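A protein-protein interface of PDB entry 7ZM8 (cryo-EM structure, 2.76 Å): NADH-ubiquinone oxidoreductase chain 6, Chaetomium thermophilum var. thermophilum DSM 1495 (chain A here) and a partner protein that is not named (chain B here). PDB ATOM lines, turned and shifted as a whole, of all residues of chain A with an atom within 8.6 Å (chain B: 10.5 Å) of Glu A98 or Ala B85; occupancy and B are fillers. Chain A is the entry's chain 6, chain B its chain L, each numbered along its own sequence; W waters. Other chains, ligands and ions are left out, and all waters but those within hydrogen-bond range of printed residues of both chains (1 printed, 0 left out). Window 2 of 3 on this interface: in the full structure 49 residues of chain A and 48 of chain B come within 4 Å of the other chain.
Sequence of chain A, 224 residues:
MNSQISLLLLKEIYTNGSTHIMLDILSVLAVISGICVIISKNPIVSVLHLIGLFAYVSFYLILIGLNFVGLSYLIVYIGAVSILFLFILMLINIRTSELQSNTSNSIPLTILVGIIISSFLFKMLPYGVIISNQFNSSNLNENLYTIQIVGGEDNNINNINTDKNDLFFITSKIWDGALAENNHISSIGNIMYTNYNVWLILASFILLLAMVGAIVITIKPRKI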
ATOM      1  N   LYS A  41       2.333  10.484 -20.481  1.00  0.00           N
ATOM      2  CA  LYS A  41       1.440   9.805 -19.548  1.00  0.00           C
ATOM      3  C   LYS A  41       0.731   8.633 -20.214  1.00  0.00           C
ATOM      4  O   LYS A  41       0.658   7.535 -19.651  1.00  0.00           O
ATOM      5  CB  LYS A  41       0.420  10.795 -18.987  1.00  0.00           C
ATOM      6  CG  LYS A  41       0.912  11.606 -17.801  1.00  0.00           C
ATOM      7  CD  LYS A  41       1.638  12.864 -18.248  1.00  0.00           C
ATOM      8  CE  LYS A  41       1.925  13.778 -17.066  1.00  0.00           C
ATOM      9  NZ  LYS A  41       2.721  14.971 -17.461  1.00  0.00           N
ATOM     10  N   ILE A  92      -6.829  -2.939 -24.226  1.00  0.00           N
ATOM     11  CA  ILE A  92      -6.755  -3.060 -22.776  1.00  0.00           C
ATOM     12  C   ILE A  92      -7.355  -1.829 -22.107  1.00  0.00           C
ATOM     13  O   ILE A  92      -7.221  -0.697 -22.586  1.00  0.00           O
ATOM     14  CB  ILE A  92      -5.300  -3.292 -22.329  1.00  0.00           C
ATOM     15  CG1 ILE A  92      -4.880  -4.740 -22.592  1.00  0.00           C
ATOM     16  CG2 ILE A  92      -5.073  -2.859 -20.898  1.00  0.00           C
ATOM     17  CD1 ILE A  92      -3.426  -5.014 -22.296  1.00  0.00           C
ATOM     18  N   ASN A  93      -8.048  -2.058 -20.996  1.00  0.00           N
ATOM     19  CA  ASN A  93      -8.545  -0.971 -20.162  1.00  0.00           C
ATOM     20  C   ASN A  93      -7.366  -0.347 -19.436  1.00  0.00           C
ATOM     21  O   ASN A  93      -6.755  -0.978 -18.572  1.00  0.00           O
ATOM     22  CB  ASN A  93      -9.589  -1.488 -19.178  1.00  0.00           C
ATOM     23  CG  ASN A  93     -10.909  -1.796 -19.845  1.00  0.00           C
ATOM     24  OD1 ASN A  93     -11.349  -2.944 -19.874  1.00  0.00           O
ATOM     25  ND2 ASN A  93     -11.547  -0.770 -20.394  1.00  0.00           N
ATOM     26  N   ILE A  94      -7.041   0.893 -19.783  1.00  0.00           N
ATOM     27  CA  ILE A  94      -5.924   1.613 -19.190  1.00  0.00           C
ATOM     28  C   ILE A  94      -6.475   2.832 -18.473  1.00  0.00           C
ATOM     29  O   ILE A  94      -7.121   3.687 -19.091  1.00  0.00           O
ATOM     30  CB  ILE A  94      -4.884   2.024 -20.244  1.00  0.00           C
ATOM     31  CG1 ILE A  94      -4.177   0.797 -20.815  1.00  0.00           C
ATOM     32  CG2 ILE A  94      -3.880   2.985 -19.647  1.00  0.00           C
ATOM     33  CD1 ILE A  94      -3.804   0.929 -22.263  1.00  0.00           C
ATOM     34  N   ARG A  95      -6.218   2.917 -17.175  1.00  0.00           N
ATOM     35  CA  ARG A  95      -6.475   4.126 -16.410  1.00  0.00           C
ATOM     36  C   ARG A  95      -5.157   4.878 -16.276  1.00  0.00           C
ATOM     37  O   ARG A  95      -4.190   4.352 -15.716  1.00  0.00           O
ATOM     38  CB  ARG A  95      -7.073   3.800 -15.045  1.00  0.00           C
ATOM     39  CG  ARG A  95      -8.568   3.555 -15.095  1.00  0.00           C
ATOM     40  CD  ARG A  95      -9.197   3.599 -13.717  1.00  0.00           C
ATOM     41  NE  ARG A  95      -9.608   2.272 -13.274  1.00  0.00           N
ATOM     42  CZ  ARG A  95     -10.850   1.809 -13.360  1.00  0.00           C
ATOM     43  NH1 ARG A  95     -11.137   0.587 -12.934  1.00  0.00           N
ATOM     44  NH2 ARG A  95     -11.807   2.568 -13.877  1.00  0.00           N
ATOM     45  N   THR A  96      -5.120   6.100 -16.807  1.00  0.00           N
ATOM     46  CA  THR A  96      -3.861   6.821 -16.933  1.00  0.00           C
ATOM     47  C   THR A  96      -3.334   7.319 -15.597  1.00  0.00           C
ATOM     48  O   THR A  96      -2.124   7.523 -15.462  1.00  0.00           O
ATOM     49  CB  THR A  96      -4.024   7.990 -17.906  1.00  0.00           C
ATOM     50  OG1 THR A  96      -2.740   8.546 -18.212  1.00  0.00           O
ATOM     51  CG2 THR A  96      -4.914   9.070 -17.311  1.00  0.00           C
ATOM     52  N   SER A  97      -4.205   7.520 -14.609  1.00  0.00           N
ATOM     53  CA  SER A  97      -3.747   7.959 -13.300  1.00  0.00           C
ATOM     54  C   SER A  97      -2.962   6.879 -12.574  1.00  0.00           C
ATOM     55  O   SER A  97      -2.103   7.203 -11.749  1.00  0.00           O
ATOM     56  CB  SER A  97      -4.937   8.400 -12.452  1.00  0.00           C
ATOM     57  OG  SER A  97      -4.529   8.746 -11.141  1.00  0.00           O
ATOM     58  N   GLU A  98      -3.228   5.610 -12.864  1.00  0.00           N
ATOM     59  CA  GLU A  98      -2.538   4.519 -12.197  1.00  0.00           C
ATOM     60  C   GLU A  98      -1.176   4.213 -12.802  1.00  0.00           C
ATOM     61  O   GLU A  98      -0.440   3.391 -12.249  1.00  0.00           O
ATOM     62  CB  GLU A  98      -3.403   3.255 -12.221  1.00  0.00           C
ATOM     63  CG  GLU A  98      -4.795   3.449 -11.664  1.00  0.00           C
ATOM     64  CD  GLU A  98      -5.792   2.449 -12.215  1.00  0.00           C
ATOM     65  OE1 GLU A  98      -5.411   1.634 -13.081  1.00  0.00           O
ATOM     66  OE2 GLU A  98      -6.959   2.469 -11.774  1.00  0.00           O
ATOM     67  N   LEU A  99      -0.824   4.845 -13.917  1.00  0.00           N
ATOM     68  CA  LEU A  99       0.465   4.632 -14.550  1.00  0.00           C
ATOM     69  C   LEU A  99       1.424   5.786 -14.319  1.00  0.00           C
ATOM     70  O   LEU A  99       2.580   5.711 -14.746  1.00  0.00           O
ATOM     71  CB  LEU A  99       0.284   4.399 -16.051  1.00  0.00           C
ATOM     72  CG  LEU A  99      -0.406   3.085 -16.403  1.00  0.00           C
ATOM     73  CD1 LEU A  99      -0.717   3.034 -17.879  1.00  0.00           C
ATOM     74  CD2 LEU A  99       0.436   1.896 -15.985  1.00  0.00           C
ATOM     75  N   GLN A 100       0.979   6.840 -13.645  1.00  0.00           N
ATOM     76  CA  GLN A 100       1.786   8.020 -13.397  1.00  0.00           C
ATOM     77  C   GLN A 100       2.457   7.900 -12.038  1.00  0.00           C
ATOM     78  O   GLN A 100       1.799   7.582 -11.041  1.00  0.00           O
ATOM     79  CB  GLN A 100       0.927   9.285 -13.455  1.00  0.00           C
ATOM     80  CG  GLN A 100       1.707  10.569 -13.255  1.00  0.00           C
ATOM     81  CD  GLN A 100       2.852  10.706 -14.235  1.00  0.00           C
ATOM     82  OE1 GLN A 100       2.718  10.378 -15.413  1.00  0.00           O
ATOM     83  NE2 GLN A 100       3.989  11.190 -13.750  1.00  0.00           N
ATOM     84  N   SER A 101       3.759   8.148 -12.004  1.00  0.00           N
ATOM     85  CA  SER A 101       4.540   8.129 -10.779  1.00  0.00           C
ATOM     86  C   SER A 101       5.236   9.472 -10.605  1.00  0.00           C
ATOM     87  O   SER A 101       5.400  10.242 -11.553  1.00  0.00           O
ATOM     88  CB  SER A 101       5.564   6.989 -10.797  1.00  0.00           C
ATOM     89  OG  SER A 101       6.593   7.246 -11.735  1.00  0.00           O
ATOM     90  N   ASN B  18      10.478   4.730 -14.220  1.00  0.00           N
ATOM     91  CA  ASN B  18       9.263   3.937 -14.375  1.00  0.00           C
ATOM     92  C   ASN B  18       8.951   3.184 -13.092  1.00  0.00           C
ATOM     93  O   ASN B  18       9.657   2.239 -12.733  1.00  0.00           O
ATOM     94  CB  ASN B  18       9.397   2.968 -15.541  1.00  0.00           C
ATOM     95  CG  ASN B  18       8.062   2.545 -16.083  1.00  0.00           C
ATOM     96  OD1 ASN B  18       7.036   3.119 -15.732  1.00  0.00           O
ATOM     97  ND2 ASN B  18       8.060   1.531 -16.931  1.00  0.00           N
ATOM     98  N   ARG B  19       7.868   3.582 -12.424  1.00  0.00           N
ATOM     99  CA  ARG B  19       7.342   2.844 -11.290  1.00  0.00           C
ATOM    100  C   ARG B  19       6.037   2.124 -11.583  1.00  0.00           C
ATOM    101  O   ARG B  19       5.660   1.234 -10.817  1.00  0.00           O
ATOM    102  CB  ARG B  19       7.112   3.784 -10.098  1.00  0.00           C
ATOM    103  CG  ARG B  19       8.342   4.496  -9.606  1.00  0.00           C
ATOM    104  CD  ARG B  19       9.174   3.615  -8.689  1.00  0.00           C
ATOM    105  NE  ARG B  19      10.059   2.714  -9.423  1.00  0.00           N
ATOM    106  CZ  ARG B  19      11.112   3.104 -10.132  1.00  0.00           C
ATOM    107  NH1 ARG B  19      11.854   2.206 -10.760  1.00  0.00           N
ATOM    108  NH2 ARG B  19      11.427   4.388 -10.212  1.00  0.00           N
ATOM    109  N   LYS B  20       5.336   2.483 -12.658  1.00  0.00           N
ATOM    110  CA  LYS B  20       3.996   1.952 -12.862  1.00  0.00           C
ATOM    111  C   LYS B  20       3.794   1.311 -14.231  1.00  0.00           C
ATOM    112  O   LYS B  20       3.100   0.296 -14.340  1.00  0.00           O
ATOM    113  CB  LYS B  20       2.968   3.063 -12.659  1.00  0.00           C
ATOM    114  CG  LYS B  20       3.220   3.947 -11.452  1.00  0.00           C
ATOM    115  CD  LYS B  20       2.594   3.362 -10.201  1.00  0.00           C
ATOM    116  CE  LYS B  20       2.277   4.447  -9.185  1.00  0.00           C
ATOM    117  NZ  LYS B  20       1.120   5.283  -9.611  1.00  0.00           N
ATOM    118  N   ASN B  21       4.375   1.892 -15.278  1.00  0.00           N
ATOM    119  CA  ASN B  21       4.209   1.378 -16.636  1.00  0.00           C
ATOM    120  C   ASN B  21       5.017   0.102 -16.806  1.00  0.00           C
ATOM    121  O   ASN B  21       6.249   0.138 -16.803  1.00  0.00           O
ATOM    122  CB  ASN B  21       4.668   2.397 -17.673  1.00  0.00           C
ATOM    123  CG  ASN B  21       3.729   3.539 -17.838  1.00  0.00           C
ATOM    124  OD1 ASN B  21       2.524   3.354 -17.910  1.00  0.00           O
ATOM    125  ND2 ASN B  21       4.272   4.742 -17.891  1.00  0.00           N
ATOM    126  N   ILE B  22       4.333  -1.022 -16.988  1.00  0.00           N
ATOM    127  CA  ILE B  22       5.017  -2.189 -17.522  1.00  0.00           C
ATOM    128  C   ILE B  22       4.967  -2.195 -19.043  1.00  0.00           C
ATOM    129  O   ILE B  22       5.706  -2.960 -19.673  1.00  0.00           O
ATOM    130  CB  ILE B  22       4.447  -3.497 -16.949  1.00  0.00           C
ATOM    131  CG1 ILE B  22       3.074  -3.804 -17.527  1.00  0.00           C
ATOM    132  CG2 ILE B  22       4.348  -3.392 -15.456  1.00  0.00           C
ATOM    133  CD1 ILE B  22       2.585  -5.177 -17.174  1.00  0.00           C
ATOM    134  N   ILE B  23       4.122  -1.356 -19.646  1.00  0.00           N
ATOM    135  CA  ILE B  23       4.172  -1.147 -21.088  1.00  0.00           C
ATOM    136  C   ILE B  23       5.427  -0.375 -21.466  1.00  0.00           C
ATOM    137  O   ILE B  23       6.087  -0.686 -22.461  1.00  0.00           O
ATOM    138  CB  ILE B  23       2.899  -0.425 -21.566  1.00  0.00           C
ATOM    139  CG1 ILE B  23       1.673  -1.307 -21.361  1.00  0.00           C
ATOM    140  CG2 ILE B  23       3.011  -0.059 -23.036  1.00  0.00           C
ATOM    141  CD1 ILE B  23       1.702  -2.562 -22.170  1.00  0.00           C
ATOM    142  N   LEU B  24       5.781   0.637 -20.676  1.00  0.00           N
ATOM    143  CA  LEU B  24       6.949   1.446 -20.989  1.00  0.00           C
ATOM    144  C   LEU B  24       8.250   0.669 -20.816  1.00  0.00           C
ATOM    145  O   LEU B  24       9.267   1.050 -21.402  1.00  0.00           O
ATOM    146  CB  LEU B  24       6.945   2.710 -20.132  1.00  0.00           C
ATOM    147  CG  LEU B  24       7.983   3.815 -20.301  1.00  0.00           C
ATOM    148  CD1 LEU B  24       7.930   4.409 -21.700  1.00  0.00           C
ATOM    149  CD2 LEU B  24       7.748   4.885 -19.252  1.00  0.00           C
ATOM    150  N   MET B  25       8.250  -0.418 -20.032  1.00  0.00           N
ATOM    151  CA  MET B  25       9.430  -1.281 -20.016  1.00  0.00           C
ATOM    152  C   MET B  25       9.542  -2.107 -21.291  1.00  0.00           C
ATOM    153  O   MET B  25      10.649  -2.428 -21.726  1.00  0.00           O
ATOM    154  CB  MET B  25       9.456  -2.203 -18.798  1.00  0.00           C
ATOM    155  CG  MET B  25       9.635  -1.513 -17.471  1.00  0.00           C
ATOM    156  SD  MET B  25       9.733  -2.728 -16.152  1.00  0.00           S
ATOM    157  CE  MET B  25       8.035  -3.226 -16.063  1.00  0.00           C
ATOM    158  N   LEU B  74       1.709 -10.727 -21.938  1.00  0.00           N
ATOM    159  CA  LEU B  74       0.948  -9.633 -21.351  1.00  0.00           C
ATOM    160  C   LEU B  74      -0.551  -9.838 -21.538  1.00  0.00           C
ATOM    161  O   LEU B  74      -1.351  -9.411 -20.702  1.00  0.00           O
ATOM    162  CB  LEU B  74       1.397  -8.309 -21.964  1.00  0.00           C
ATOM    163  CG  LEU B  74       0.685  -7.062 -21.461  1.00  0.00           C
ATOM    164  CD1 LEU B  74       1.322  -6.570 -20.188  1.00  0.00           C
ATOM    165  CD2 LEU B  74       0.692  -5.990 -22.527  1.00  0.00           C
ATOM    166  N   PHE B  77      -1.596 -12.466 -18.923  1.00  0.00           N
ATOM    167  CA  PHE B  77      -1.656 -11.796 -17.603  1.00  0.00           C
ATOM    168  C   PHE B  77      -2.918 -10.937 -17.455  1.00  0.00           C
ATOM    169  O   PHE B  77      -3.584 -11.051 -16.419  1.00  0.00           O
ATOM    170  CB  PHE B  77      -0.370 -10.984 -17.449  1.00  0.00           C
ATOM    171  CG  PHE B  77      -0.236 -10.158 -16.200  1.00  0.00           C
ATOM    172  CD1 PHE B  77       0.153 -10.737 -15.007  1.00  0.00           C
ATOM    173  CD2 PHE B  77      -0.464  -8.793 -16.233  1.00  0.00           C
ATOM    174  CE1 PHE B  77       0.292  -9.969 -13.865  1.00  0.00           C
ATOM    175  CE2 PHE B  77      -0.328  -8.027 -15.089  1.00  0.00           C
ATOM    176  CZ  PHE B  77       0.055  -8.617 -13.912  1.00  0.00           C
ATOM    177  N   TYR B  78      -3.264 -10.148 -18.472  1.00  0.00           N
ATOM    178  CA  TYR B  78      -4.456  -9.259 -18.450  1.00  0.00           C
ATOM    179  C   TYR B  78      -5.761 -10.052 -18.341  1.00  0.00           C
ATOM    180  O   TYR B  78      -6.664  -9.573 -17.656  1.00  0.00           O
ATOM    181  CB  TYR B  78      -4.442  -8.347 -19.682  1.00  0.00           C
ATOM    182  CG  TYR B  78      -5.561  -7.342 -19.728  1.00  0.00           C
ATOM    183  CD1 TYR B  78      -5.539  -6.216 -18.925  1.00  0.00           C
ATOM    184  CD2 TYR B  78      -6.642  -7.523 -20.569  1.00  0.00           C
ATOM    185  CE1 TYR B  78      -6.573  -5.298 -18.948  1.00  0.00           C
ATOM    186  CE2 TYR B  78      -7.682  -6.615 -20.607  1.00  0.00           C
ATOM    187  CZ  TYR B  78      -7.646  -5.498 -19.794  1.00  0.00           C
ATOM    188  OH  TYR B  78      -8.672  -4.602 -19.836  1.00  0.00           O
ATOM    189  N   ARG B  81      -6.100 -10.740 -14.682  1.00  0.00           N
ATOM    190  CA  ARG B  81      -5.889  -9.649 -13.692  1.00  0.00           C
ATOM    191  C   ARG B  81      -6.815  -8.462 -13.964  1.00  0.00           C
ATOM    192  O   ARG B  81      -7.332  -7.891 -12.995  1.00  0.00           O
ATOM    193  CB  ARG B  81      -4.403  -9.285 -13.596  1.00  0.00           C
ATOM    194  CG  ARG B  81      -4.038  -8.454 -12.378  1.00  0.00           C
ATOM    195  CD  ARG B  81      -2.635  -8.800 -11.939  1.00  0.00           C
ATOM    196  NE  ARG B  81      -2.120  -7.998 -10.842  1.00  0.00           N
ATOM    197  CZ  ARG B  81      -2.095  -8.382  -9.572  1.00  0.00           C
ATOM    198  NH1 ARG B  81      -2.555  -9.572  -9.229  1.00  0.00           N
ATOM    199  NH2 ARG B  81      -1.601  -7.577  -8.650  1.00  0.00           N
ATOM    200  N   GLY B  82      -7.016  -8.101 -15.227  1.00  0.00           N
ATOM    201  CA  GLY B  82      -7.962  -7.024 -15.576  1.00  0.00           C
ATOM    202  C   GLY B  82      -7.337  -5.659 -15.524  1.00  0.00           C
ATOM    203  O   GLY B  82      -8.041  -4.685 -15.771  1.00  0.00           O
ATOM    204  N   SER B  83      -6.061  -5.603 -15.185  1.00  0.00           N
ATOM    205  CA  SER B  83      -5.321  -4.326 -15.139  1.00  0.00           C
ATOM    206  C   SER B  83      -3.865  -4.632 -15.447  1.00  0.00           C
ATOM    207  O   SER B  83      -3.425  -5.739 -15.127  1.00  0.00           O
ATOM    208  CB  SER B  83      -5.461  -3.666 -13.800  1.00  0.00           C
ATOM    209  OG  SER B  83      -5.096  -4.555 -12.759  1.00  0.00           O
ATOM    210  N   ILE B  84      -3.161  -3.692 -16.058  1.00  0.00           N
ATOM    211  CA  ILE B  84      -1.710  -3.882 -16.287  1.00  0.00           C
ATOM    212  C   ILE B  84      -1.025  -2.864 -15.390  1.00  0.00           C
ATOM    213  O   ILE B  84       0.079  -2.417 -15.743  1.00  0.00           O
ATOM    214  CB  ILE B  84      -1.375  -3.673 -17.775  1.00  0.00           C
ATOM    215  CG1 ILE B  84      -1.935  -2.357 -18.315  1.00  0.00           C
ATOM    216  CG2 ILE B  84      -1.847  -4.860 -18.600  1.00  0.00           C
ATOM    217  CD1 ILE B  84      -1.644  -2.135 -19.776  1.00  0.00           C
ATOM    218  N   ALA B  85      -1.647  -2.537 -14.257  1.00  0.00           N
ATOM    219  CA  ALA B  85      -1.115  -1.486 -13.408  1.00  0.00           C
ATOM    220  C   ALA B  85      -0.494  -2.091 -12.160  1.00  0.00           C
ATOM    221  O   ALA B  85      -1.032  -3.043 -11.589  1.00  0.00           O
ATOM    222  CB  ALA B  85      -2.212  -0.493 -13.020  1.00  0.00           C
ATOM    223  N   ILE B  86       0.649  -1.540 -11.747  1.00  0.00           N
ATOM    224  CA  ILE B  86       1.279  -1.990 -10.513  1.00  0.00           C
ATOM    225  C   ILE B  86       0.787  -1.147  -9.341  1.00  0.00           C
ATOM    226  O   ILE B  86       0.815   0.088  -9.362  1.00  0.00           O
ATOM    227  CB  ILE B  86       2.813  -1.948 -10.623  1.00  0.00           C
ATOM    228  CG1 ILE B  86       3.302  -2.974 -11.639  1.00  0.00           C
ATOM    229  CG2 ILE B  86       3.462  -2.201  -9.275  1.00  0.00           C
ATOM    230  CD1 ILE B  86       4.754  -2.825 -11.998  1.00  0.00           C
ATOM    231  N   GLU B  87       0.332  -1.835  -8.297  1.00  0.00           N
ATOM    232  CA  GLU B  87      -0.205  -1.192  -7.098  1.00  0.00           C
ATOM    233  C   GLU B  87       0.977  -0.678  -6.282  1.00  0.00           C
ATOM    234  O   GLU B  87       1.514  -1.374  -5.421  1.00  0.00           O
ATOM    235  CB  GLU B  87      -1.066  -2.163  -6.302  1.00  0.00           C
ATOM    236  CG  GLU B  87      -1.703  -1.561  -5.063  1.00  0.00           C
ATOM    237  CD  GLU B  87      -2.728  -0.495  -5.392  1.00  0.00           C
ATOM    238  OE1 GLU B  87      -3.363  -0.589  -6.463  1.00  0.00           O
ATOM    239  OE2 GLU B  87      -2.903   0.436  -4.578  1.00  0.00           O
ATOM    240  N   TYR B  88       1.381   0.556  -6.560  1.00  0.00           N
ATOM    241  CA  TYR B  88       2.541   1.151  -5.908  1.00  0.00           C
ATOM    242  C   TYR B  88       2.127   2.224  -4.909  1.00  0.00           C
ATOM    243  O   TYR B  88       1.883   1.936  -3.739  1.00  0.00           O
ATOM    244  CB  TYR B  88       3.487   1.741  -6.953  1.00  0.00           C
ATOM    245  CG  TYR B  88       4.922   1.851  -6.498  1.00  0.00           C
ATOM    246  CD1 TYR B  88       5.648   0.719  -6.151  1.00  0.00           C
ATOM    247  CD2 TYR B  88       5.556   3.081  -6.427  1.00  0.00           C
ATOM    248  CE1 TYR B  88       6.960   0.812  -5.740  1.00  0.00           C
ATOM    249  CE2 TYR B  88       6.867   3.187  -6.014  1.00  0.00           C
ATOM    250  CZ  TYR B  88       7.565   2.049  -5.671  1.00  0.00           C
ATOM    251  OH  TYR B  88       8.874   2.152  -5.263  1.00  0.00           O
HETATM  252  O   HOH W   1      -7.162  -1.673 -16.105  1.00  0.00           O
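No residue of chain B comes within 4 Å of Thr A96. Ser A97 touches none of the printed residues of chain B. Printed residues of chain B within 4 Å of Gln A100: Lys B20 (2.8 Å). Printed residues of chain B within 4 Å of Ser A101: Arg B19 (3.6 Å) and Lys B20 (3.9 Å). Of the printed residues of chain A, Lys B20 touches Glu A98, Leu A99, Gln A100 and Ser A101. Of the printed residues of chain A, Asn B21 touches Leu A99. Met B25 touches none of the printed residues of chain A. Ala B85 touches one residue of chain A. The nearest residue of chain B that does not touch Glu A98 is Ile B86 (4.6 Å).
Water W1 lies within hydrogen-bond range of the backbone carbonyl oxygen of Asn A93 (2.6 Å) and the backbone carbonyl oxygen of Gly B82 (3.2 Å).
The side-chain amide oxygen (OD1) of Asn B18 lies within hydrogen-bond range of the backbone NH (N) of Asn B21, 3.0 Å away. NE of Arg A95 lies within salt-bridge range of OE2 of Glu A98, at 3.1 Å.
Of the 19 printed residues of chain B, 6 touch a printed residue of chain A. Hydrophobic or aromatic side chains of chain B that line the printed part of chain A: Tyr B78, Ile B84 and Ala B85.
CG2 of Ile A92 touches CE1 of Tyr B78, 3.5 Å away. Ile A92 touches Ile B84. O of Glu A98 touches CB of Lys B20, at 3.4 Å. Glu A98 touches Ala B85. O of Leu A99 touches CB of Lys B20, at 3.4 Å. Asn B21 touches Leu A99. CB of Ser A101 touches CB of Arg B19, at 3.6 Å. Lys B20 touches Ser A101.
OH of Tyr B78 is in hydrogen-bond range of N of Asn A93. The side-chain amino group (NZ) of Lys B20 lies within hydrogen-bond range of the backbone carbonyl oxygen (O) of Gln A100 (2.8 Å).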
